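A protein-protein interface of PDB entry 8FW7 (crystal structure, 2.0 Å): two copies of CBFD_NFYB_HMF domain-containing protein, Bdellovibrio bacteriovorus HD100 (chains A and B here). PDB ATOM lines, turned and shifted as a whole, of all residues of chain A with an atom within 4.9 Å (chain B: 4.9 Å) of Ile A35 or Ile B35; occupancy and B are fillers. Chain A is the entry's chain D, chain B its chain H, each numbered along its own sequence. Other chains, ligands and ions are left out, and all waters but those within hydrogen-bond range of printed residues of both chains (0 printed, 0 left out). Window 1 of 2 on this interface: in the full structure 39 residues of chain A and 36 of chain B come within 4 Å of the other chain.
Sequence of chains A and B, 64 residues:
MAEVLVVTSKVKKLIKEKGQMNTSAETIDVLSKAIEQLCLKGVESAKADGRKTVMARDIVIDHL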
ATOM      1  N   LEU A   5     -28.643 -13.241  20.004  1.00  0.00           N
ATOM      2  CA  LEU A   5     -27.937 -12.210  19.257  1.00  0.00           C
ATOM      3  C   LEU A   5     -27.038 -12.783  18.172  1.00  0.00           C
ATOM      4  O   LEU A   5     -26.391 -12.018  17.448  1.00  0.00           O
ATOM      5  CB  LEU A   5     -27.124 -11.340  20.223  1.00  0.00           C
ATOM      6  CG  LEU A   5     -27.915 -10.641  21.337  1.00  0.00           C
ATOM      7  CD1 LEU A   5     -26.923  -9.915  22.248  1.00  0.00           C
ATOM      8  CD2 LEU A   5     -28.935  -9.642  20.770  1.00  0.00           C
ATOM      9  N   VAL A   6     -26.990 -14.105  18.029  1.00  0.00           N
ATOM     10  CA  VAL A   6     -26.200 -14.737  16.981  1.00  0.00           C
ATOM     11  C   VAL A   6     -27.150 -15.396  15.986  1.00  0.00           C
ATOM     12  O   VAL A   6     -28.283 -15.745  16.314  1.00  0.00           O
ATOM     13  CB  VAL A   6     -25.190 -15.769  17.530  1.00  0.00           C
ATOM     14  CG1 VAL A   6     -24.222 -15.116  18.502  1.00  0.00           C
ATOM     15  CG2 VAL A   6     -25.918 -16.924  18.187  1.00  0.00           C
ATOM     16  N   VAL A  11     -23.963 -20.136  12.628  1.00  0.00           N
ATOM     17  CA  VAL A  11     -23.027 -20.625  13.638  1.00  0.00           C
ATOM     18  C   VAL A  11     -22.893 -22.143  13.526  1.00  0.00           C
ATOM     19  O   VAL A  11     -21.784 -22.683  13.420  1.00  0.00           O
ATOM     20  CB  VAL A  11     -23.480 -20.187  15.042  1.00  0.00           C
ATOM     21  CG1 VAL A  11     -22.772 -21.017  16.128  1.00  0.00           C
ATOM     22  CG2 VAL A  11     -23.213 -18.682  15.233  1.00  0.00           C
ATOM     23  N   LEU A  31     -22.723 -17.813  23.473  1.00  0.00           N
ATOM     24  CA  LEU A  31     -22.203 -16.956  22.412  1.00  0.00           C
ATOM     25  C   LEU A  31     -22.925 -15.613  22.418  1.00  0.00           C
ATOM     26  O   LEU A  31     -22.299 -14.557  22.258  1.00  0.00           O
ATOM     27  CB  LEU A  31     -22.354 -17.653  21.056  1.00  0.00           C
ATOM     28  CG  LEU A  31     -21.303 -18.697  20.634  1.00  0.00           C
ATOM     29  CD1 LEU A  31     -21.675 -19.391  19.322  1.00  0.00           C
ATOM     30  CD2 LEU A  31     -19.907 -18.084  20.536  1.00  0.00           C
ATOM     31  N   SER A  32     -24.246 -15.650  22.615  1.00  0.00           N
ATOM     32  CA  SER A  32     -25.055 -14.442  22.720  1.00  0.00           C
ATOM     33  C   SER A  32     -24.667 -13.606  23.938  1.00  0.00           C
ATOM     34  O   SER A  32     -24.576 -12.374  23.850  1.00  0.00           O
ATOM     35  CB  SER A  32     -26.535 -14.842  22.757  1.00  0.00           C
ATOM     36  OG  SER A  32     -27.382 -13.714  22.638  1.00  0.00           O
ATOM     37  N   LYS A  33     -24.403 -14.254  25.078  1.00  0.00           N
ATOM     38  CA  LYS A  33     -23.938 -13.516  26.256  1.00  0.00           C
ATOM     39  C   LYS A  33     -22.616 -12.801  25.978  1.00  0.00           C
ATOM     40  O   LYS A  33     -22.413 -11.661  26.420  1.00  0.00           O
ATOM     41  CB  LYS A  33     -23.797 -14.464  27.455  1.00  0.00           C
ATOM     42  CG  LYS A  33     -23.364 -13.767  28.757  1.00  0.00           C
ATOM     43  CD  LYS A  33     -24.560 -13.161  29.471  1.00  0.00           C
ATOM     44  CE  LYS A  33     -24.159 -12.279  30.647  1.00  0.00           C
ATOM     45  NZ  LYS A  33     -23.121 -12.931  31.498  1.00  0.00           N
ATOM     46  N   ALA A  34     -21.706 -13.462  25.256  1.00  0.00           N
ATOM     47  CA  ALA A  34     -20.434 -12.840  24.899  1.00  0.00           C
ATOM     48  C   ALA A  34     -20.653 -11.599  24.056  1.00  0.00           C
ATOM     49  O   ALA A  34     -19.938 -10.606  24.212  1.00  0.00           O
ATOM     50  CB  ALA A  34     -19.551 -13.837  24.146  1.00  0.00           C
ATOM     51  N   ILE A  35     -21.648 -11.630  23.162  1.00  0.00           N
ATOM     52  CA  ILE A  35     -21.971 -10.447  22.365  1.00  0.00           C
ATOM     53  C   ILE A  35     -22.454  -9.318  23.256  1.00  0.00           C
ATOM     54  O   ILE A  35     -22.030  -8.165  23.096  1.00  0.00           O
ATOM     55  CB  ILE A  35     -23.015 -10.775  21.285  1.00  0.00           C
ATOM     56  CG1 ILE A  35     -22.388 -11.668  20.223  1.00  0.00           C
ATOM     57  CG2 ILE A  35     -23.527  -9.460  20.653  1.00  0.00           C
ATOM     58  CD1 ILE A  35     -21.176 -11.025  19.587  1.00  0.00           C
ATOM     59  N   GLU A  36     -23.391  -9.617  24.172  1.00  0.00           N
ATOM     60  CA  GLU A  36     -23.881  -8.605  25.107  1.00  0.00           C
ATOM     61  C   GLU A  36     -22.740  -7.924  25.845  1.00  0.00           C
ATOM     62  O   GLU A  36     -22.748  -6.699  26.042  1.00  0.00           O
ATOM     63  CB  GLU A  36     -24.820  -9.229  26.138  1.00  0.00           C
ATOM     64  CG  GLU A  36     -26.201  -9.571  25.658  1.00  0.00           C
ATOM     65  CD  GLU A  36     -26.995 -10.337  26.712  1.00  0.00           C
ATOM     66  OE1 GLU A  36     -26.740 -10.099  27.920  1.00  0.00           O
ATOM     67  OE2 GLU A  36     -27.856 -11.175  26.340  1.00  0.00           O
ATOM     68  N   GLN A  37     -21.756  -8.708  26.289  1.00  0.00           N
ATOM     69  CA  GLN A  37     -20.660  -8.142  27.071  1.00  0.00           C
ATOM     70  C   GLN A  37     -19.738  -7.290  26.205  1.00  0.00           C
ATOM     71  O   GLN A  37     -19.300  -6.214  26.630  1.00  0.00           O
ATOM     72  CB  GLN A  37     -19.880  -9.266  27.748  1.00  0.00           C
ATOM     73  CG  GLN A  37     -20.688 -10.079  28.752  1.00  0.00           C
ATOM     74  CD  GLN A  37     -21.236  -9.239  29.893  1.00  0.00           C
ATOM     75  OE1 GLN A  37     -20.476  -8.741  30.729  1.00  0.00           O
ATOM     76  NE2 GLN A  37     -22.558  -9.100  29.952  1.00  0.00           N
ATOM     77  N   LEU A  38     -19.421  -7.759  24.998  1.00  0.00           N
ATOM     78  CA  LEU A  38     -18.637  -6.949  24.070  1.00  0.00           C
ATOM     79  C   LEU A  38     -19.323  -5.621  23.764  1.00  0.00           C
ATOM     80  O   LEU A  38     -18.661  -4.578  23.685  1.00  0.00           O
ATOM     81  CB  LEU A  38     -18.393  -7.739  22.783  1.00  0.00           C
ATOM     82  CG  LEU A  38     -17.323  -8.832  22.835  1.00  0.00           C
ATOM     83  CD1 LEU A  38     -17.378  -9.626  21.544  1.00  0.00           C
ATOM     84  CD2 LEU A  38     -15.921  -8.233  23.066  1.00  0.00           C
ATOM     85  N   CYS A  39     -20.650  -5.644  23.571  1.00  0.00           N
ATOM     86  CA  CYS A  39     -21.396  -4.420  23.278  1.00  0.00           C
ATOM     87  C   CYS A  39     -21.383  -3.459  24.454  1.00  0.00           C
ATOM     88  O   CYS A  39     -21.272  -2.238  24.269  1.00  0.00           O
ATOM     89  CB  CYS A  39     -22.843  -4.760  22.914  1.00  0.00           C
ATOM     90  SG  CYS A  39     -23.011  -5.561  21.336  1.00  0.00           S
ATOM     91  N   LEU B   5     -22.422 -13.225  11.413  1.00  0.00           N
ATOM     92  CA  LEU B   5     -22.804 -14.181  12.448  1.00  0.00           C
ATOM     93  C   LEU B   5     -23.612 -13.573  13.589  1.00  0.00           C
ATOM     94  O   LEU B   5     -24.045 -14.316  14.478  1.00  0.00           O
ATOM     95  CB  LEU B   5     -21.556 -14.878  13.017  1.00  0.00           C
ATOM     96  CG  LEU B   5     -20.727 -15.649  11.991  1.00  0.00           C
ATOM     97  CD1 LEU B   5     -19.486 -16.244  12.635  1.00  0.00           C
ATOM     98  CD2 LEU B   5     -21.560 -16.736  11.324  1.00  0.00           C
ATOM     99  N   VAL B   6     -23.820 -12.257  13.599  1.00  0.00           N
ATOM    100  CA  VAL B   6     -24.626 -11.606  14.620  1.00  0.00           C
ATOM    101  C   VAL B   6     -25.909 -11.086  13.977  1.00  0.00           C
ATOM    102  O   VAL B   6     -25.973 -10.816  12.772  1.00  0.00           O
ATOM    103  CB  VAL B   6     -23.864 -10.457  15.333  1.00  0.00           C
ATOM    104  CG1 VAL B   6     -22.616 -10.999  16.037  1.00  0.00           C
ATOM    105  CG2 VAL B   6     -23.481  -9.387  14.345  1.00  0.00           C
ATOM    106  N   VAL B  11     -28.580  -6.453  17.982  1.00  0.00           N
ATOM    107  CA  VAL B  11     -27.397  -5.795  18.545  1.00  0.00           C
ATOM    108  C   VAL B  11     -27.615  -4.284  18.623  1.00  0.00           C
ATOM    109  O   VAL B  11     -27.388  -3.657  19.667  1.00  0.00           O
ATOM    110  CB  VAL B  11     -26.151  -6.152  17.717  1.00  0.00           C
ATOM    111  CG1 VAL B  11     -24.940  -5.283  18.140  1.00  0.00           C
ATOM    112  CG2 VAL B  11     -25.849  -7.654  17.870  1.00  0.00           C
ATOM    113  N   LEU B  31     -17.894  -7.787  15.673  1.00  0.00           N
ATOM    114  CA  LEU B  31     -18.620  -8.754  16.491  1.00  0.00           C
ATOM    115  C   LEU B  31     -18.752 -10.101  15.780  1.00  0.00           C
ATOM    116  O   LEU B  31     -18.593 -11.153  16.411  1.00  0.00           O
ATOM    117  CB  LEU B  31     -19.998  -8.207  16.864  1.00  0.00           C
ATOM    118  CG  LEU B  31     -20.045  -6.950  17.741  1.00  0.00           C
ATOM    119  CD1 LEU B  31     -21.474  -6.381  17.751  1.00  0.00           C
ATOM    120  CD2 LEU B  31     -19.567  -7.243  19.153  1.00  0.00           C
ATOM    121  N   SER B  32     -19.035 -10.093  14.467  1.00  0.00           N
ATOM    122  CA  SER B  32     -19.096 -11.353  13.720  1.00  0.00           C
ATOM    123  C   SER B  32     -17.756 -12.076  13.752  1.00  0.00           C
ATOM    124  O   SER B  32     -17.709 -13.309  13.826  1.00  0.00           O
ATOM    125  CB  SER B  32     -19.509 -11.115  12.263  1.00  0.00           C
ATOM    126  OG  SER B  32     -20.824 -10.616  12.170  1.00  0.00           O
ATOM    127  N   LYS B  33     -16.658 -11.328  13.673  1.00  0.00           N
ATOM    128  CA  LYS B  33     -15.347 -11.958  13.718  1.00  0.00           C
ATOM    129  C   LYS B  33     -15.051 -12.530  15.096  1.00  0.00           C
ATOM    130  O   LYS B  33     -14.401 -13.578  15.206  1.00  0.00           O
ATOM    131  CB  LYS B  33     -14.272 -10.962  13.303  1.00  0.00           C
ATOM    132  CG  LYS B  33     -12.932 -11.617  13.084  1.00  0.00           C
ATOM    133  CD  LYS B  33     -12.909 -12.371  11.745  1.00  0.00           C
ATOM    134  CE  LYS B  33     -11.795 -13.418  11.713  1.00  0.00           C
ATOM    135  NZ  LYS B  33     -10.556 -12.945  12.415  1.00  0.00           N
ATOM    136  N   ALA B  34     -15.528 -11.866  16.151  1.00  0.00           N
ATOM    137  CA  ALA B  34     -15.409 -12.416  17.494  1.00  0.00           C
ATOM    138  C   ALA B  34     -16.130 -13.757  17.605  1.00  0.00           C
ATOM    139  O   ALA B  34     -15.600 -14.697  18.208  1.00  0.00           O
ATOM    140  CB  ALA B  34     -15.951 -11.417  18.517  1.00  0.00           C
ATOM    141  N   ILE B  35     -17.336 -13.859  17.021  1.00  0.00           N
ATOM    142  CA  ILE B  35     -18.095 -15.113  17.028  1.00  0.00           C
ATOM    143  C   ILE B  35     -17.335 -16.192  16.273  1.00  0.00           C
ATOM    144  O   ILE B  35     -17.264 -17.342  16.717  1.00  0.00           O
ATOM    145  CB  ILE B  35     -19.502 -14.918  16.423  1.00  0.00           C
ATOM    146  CG1 ILE B  35     -20.459 -14.189  17.367  1.00  0.00           C
ATOM    147  CG2 ILE B  35     -20.143 -16.276  16.144  1.00  0.00           C
ATOM    148  CD1 ILE B  35     -20.306 -14.558  18.835  1.00  0.00           C
ATOM    149  N   GLU B  36     -16.778 -15.840  15.110  1.00  0.00           N
ATOM    150  CA  GLU B  36     -15.986 -16.787  14.331  1.00  0.00           C
ATOM    151  C   GLU B  36     -14.833 -17.336  15.159  1.00  0.00           C
ATOM    152  O   GLU B  36     -14.624 -18.555  15.222  1.00  0.00           O
ATOM    153  CB  GLU B  36     -15.463 -16.108  13.058  1.00  0.00           C
ATOM    154  CG  GLU B  36     -14.908 -17.053  11.981  1.00  0.00           C
ATOM    155  CD  GLU B  36     -14.132 -16.319  10.881  1.00  0.00           C
ATOM    156  OE1 GLU B  36     -14.417 -15.123  10.631  1.00  0.00           O
ATOM    157  OE2 GLU B  36     -13.249 -16.941  10.250  1.00  0.00           O
ATOM    158  N   GLN B  37     -14.086 -16.444  15.821  1.00  0.00           N
ATOM    159  CA  GLN B  37     -12.956 -16.869  16.642  1.00  0.00           C
ATOM    160  C   GLN B  37     -13.414 -17.737  17.813  1.00  0.00           C
ATOM    161  O   GLN B  37     -12.760 -18.734  18.145  1.00  0.00           O
ATOM    162  CB  GLN B  37     -12.179 -15.639  17.128  1.00  0.00           C
ATOM    163  CG  GLN B  37     -11.572 -14.816  15.990  1.00  0.00           C
ATOM    164  CD  GLN B  37     -10.991 -13.469  16.435  1.00  0.00           C
ATOM    165  OE1 GLN B  37     -10.381 -12.751  15.636  1.00  0.00           O
ATOM    166  NE2 GLN B  37     -11.178 -13.124  17.703  1.00  0.00           N
ATOM    167  N   LEU B  38     -14.554 -17.399  18.429  1.00  0.00           N
ATOM    168  CA  LEU B  38     -15.051 -18.185  19.556  1.00  0.00           C
ATOM    169  C   LEU B  38     -15.472 -19.586  19.121  1.00  0.00           C
ATOM    170  O   LEU B  38     -15.250 -20.559  19.854  1.00  0.00           O
ATOM    171  CB  LEU B  38     -16.216 -17.464  20.237  1.00  0.00           C
ATOM    172  CG  LEU B  38     -15.809 -16.302  21.156  1.00  0.00           C
ATOM    173  CD1 LEU B  38     -17.046 -15.565  21.632  1.00  0.00           C
ATOM    174  CD2 LEU B  38     -14.950 -16.773  22.340  1.00  0.00           C
ATOM    175  N   CYS B  39     -16.080 -19.719  17.942  1.00  0.00           N
ATOM    176  CA  CYS B  39     -16.468 -21.051  17.478  1.00  0.00           C
ATOM    177  C   CYS B  39     -15.247 -21.892  17.111  1.00  0.00           C
ATOM    178  O   CYS B  39     -15.197 -23.089  17.419  1.00  0.00           O
ATOM    179  CB  CYS B  39     -17.438 -20.954  16.295  1.00  0.00           C
ATOM    180  SG  CYS B  39     -19.025 -20.125  16.632  1.00  0.00           S
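N of Leu A5 is in hydrogen-bond range of OG of Ser A32 (3.0 Å).
The side-chain sulfur (SG) of Cys B39 is in hydrogen-bond range of the backbone carbonyl oxygen (O) of Ile B35 (3.3 Å).
The backbone NH of Leu B5 sits at hydrogen-bond distance from the side-chain hydroxyl of Ser B32, at 3.2 Å.
SG of Cys A39 sits at hydrogen-bond distance from O of Ile A35, 3.3 Å away.
Val B6 touches Leu A5 (CA to O, 3.4 Å).
Leu B5 touches Val A6.
CG1 of Val A11 touches SG of Cys B39 (3.9 Å).
Ile B35 touches Leu A31.
CD2 of Leu A31 touches CB of Leu B38, 3.8 Å away.
Leu A31 touches Cys B39 (CD1 to SG, 3.8 Å).
CD1 of Leu B38 touches CB of Ala A34 (3.9 Å).
Ile A35 touches Val B6 (CD1 to CG1, 3.8 Å).
CD1 of Leu A38 touches CB of Ala B34 (3.8 Å).
Cys A39 touches Leu B31 (SG to CD1, 3.99 Å).
Printed residues of chain B within 4 Å of Val A6: Leu B5 (3.3 Å) and Ile B35 (3.97 Å).
Of the printed residues of chain B, Val A11 touches Cys B39 (3.9 Å).
Of the printed residues of chain B, Ala A34 touches Leu B38.
Ile A35 touches just these residues of chain B: Val B6 and Ile B35.
Of the printed residues of chain B, Leu A38 touches Leu B31 (3.8 Å) and Ala B34 (3.8 Å).
Printed residues of chain A within 4 Å of Val B11: Cys A39.
Printed residues of chain A within 4 Å of Ile B35: Val A6, Leu A31 and Ile A35.
Gln B37 touches none of the printed residues of chain A.
The nearest printed residue of chain A that does not touch Ile B35 is Val A11 (4.01 Å).
Hydrophobic or aromatic side chains of chain B that line the printed part of chain A: Val B6, Val B11, Leu B31, Ala B34, Ile B35 and Leu B38.
Of the 12 printed residues of chain A, 8 touch a printed residue of chain B.
Hydrophobic or aromatic side chains of chain A within 4 Å of the printed part of chain B: Val A6, Val A11, Leu A31, Ala A34, Ile A35 and Leu A38.
Among the printed residues, 14 pairs touch across the chains.
Leu A5 touches Val B6, and with the chains exchanged Val A6 touches Leu B5.
Leu A31 touches Ile B35, but with the chains exchanged Ile A35 does not touch Leu B31 (4.1 Å).
Leu A31 touches Leu B38, and with the chains exchanged Leu A38 touches Leu B31.
Leu A31 touches Cys B39, and with the chains exchanged Cys A39 touches Leu B31.
Of the 14 pairs that touch across the chains among the printed residues, 13 have their exchanged pair printed and touching as well.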
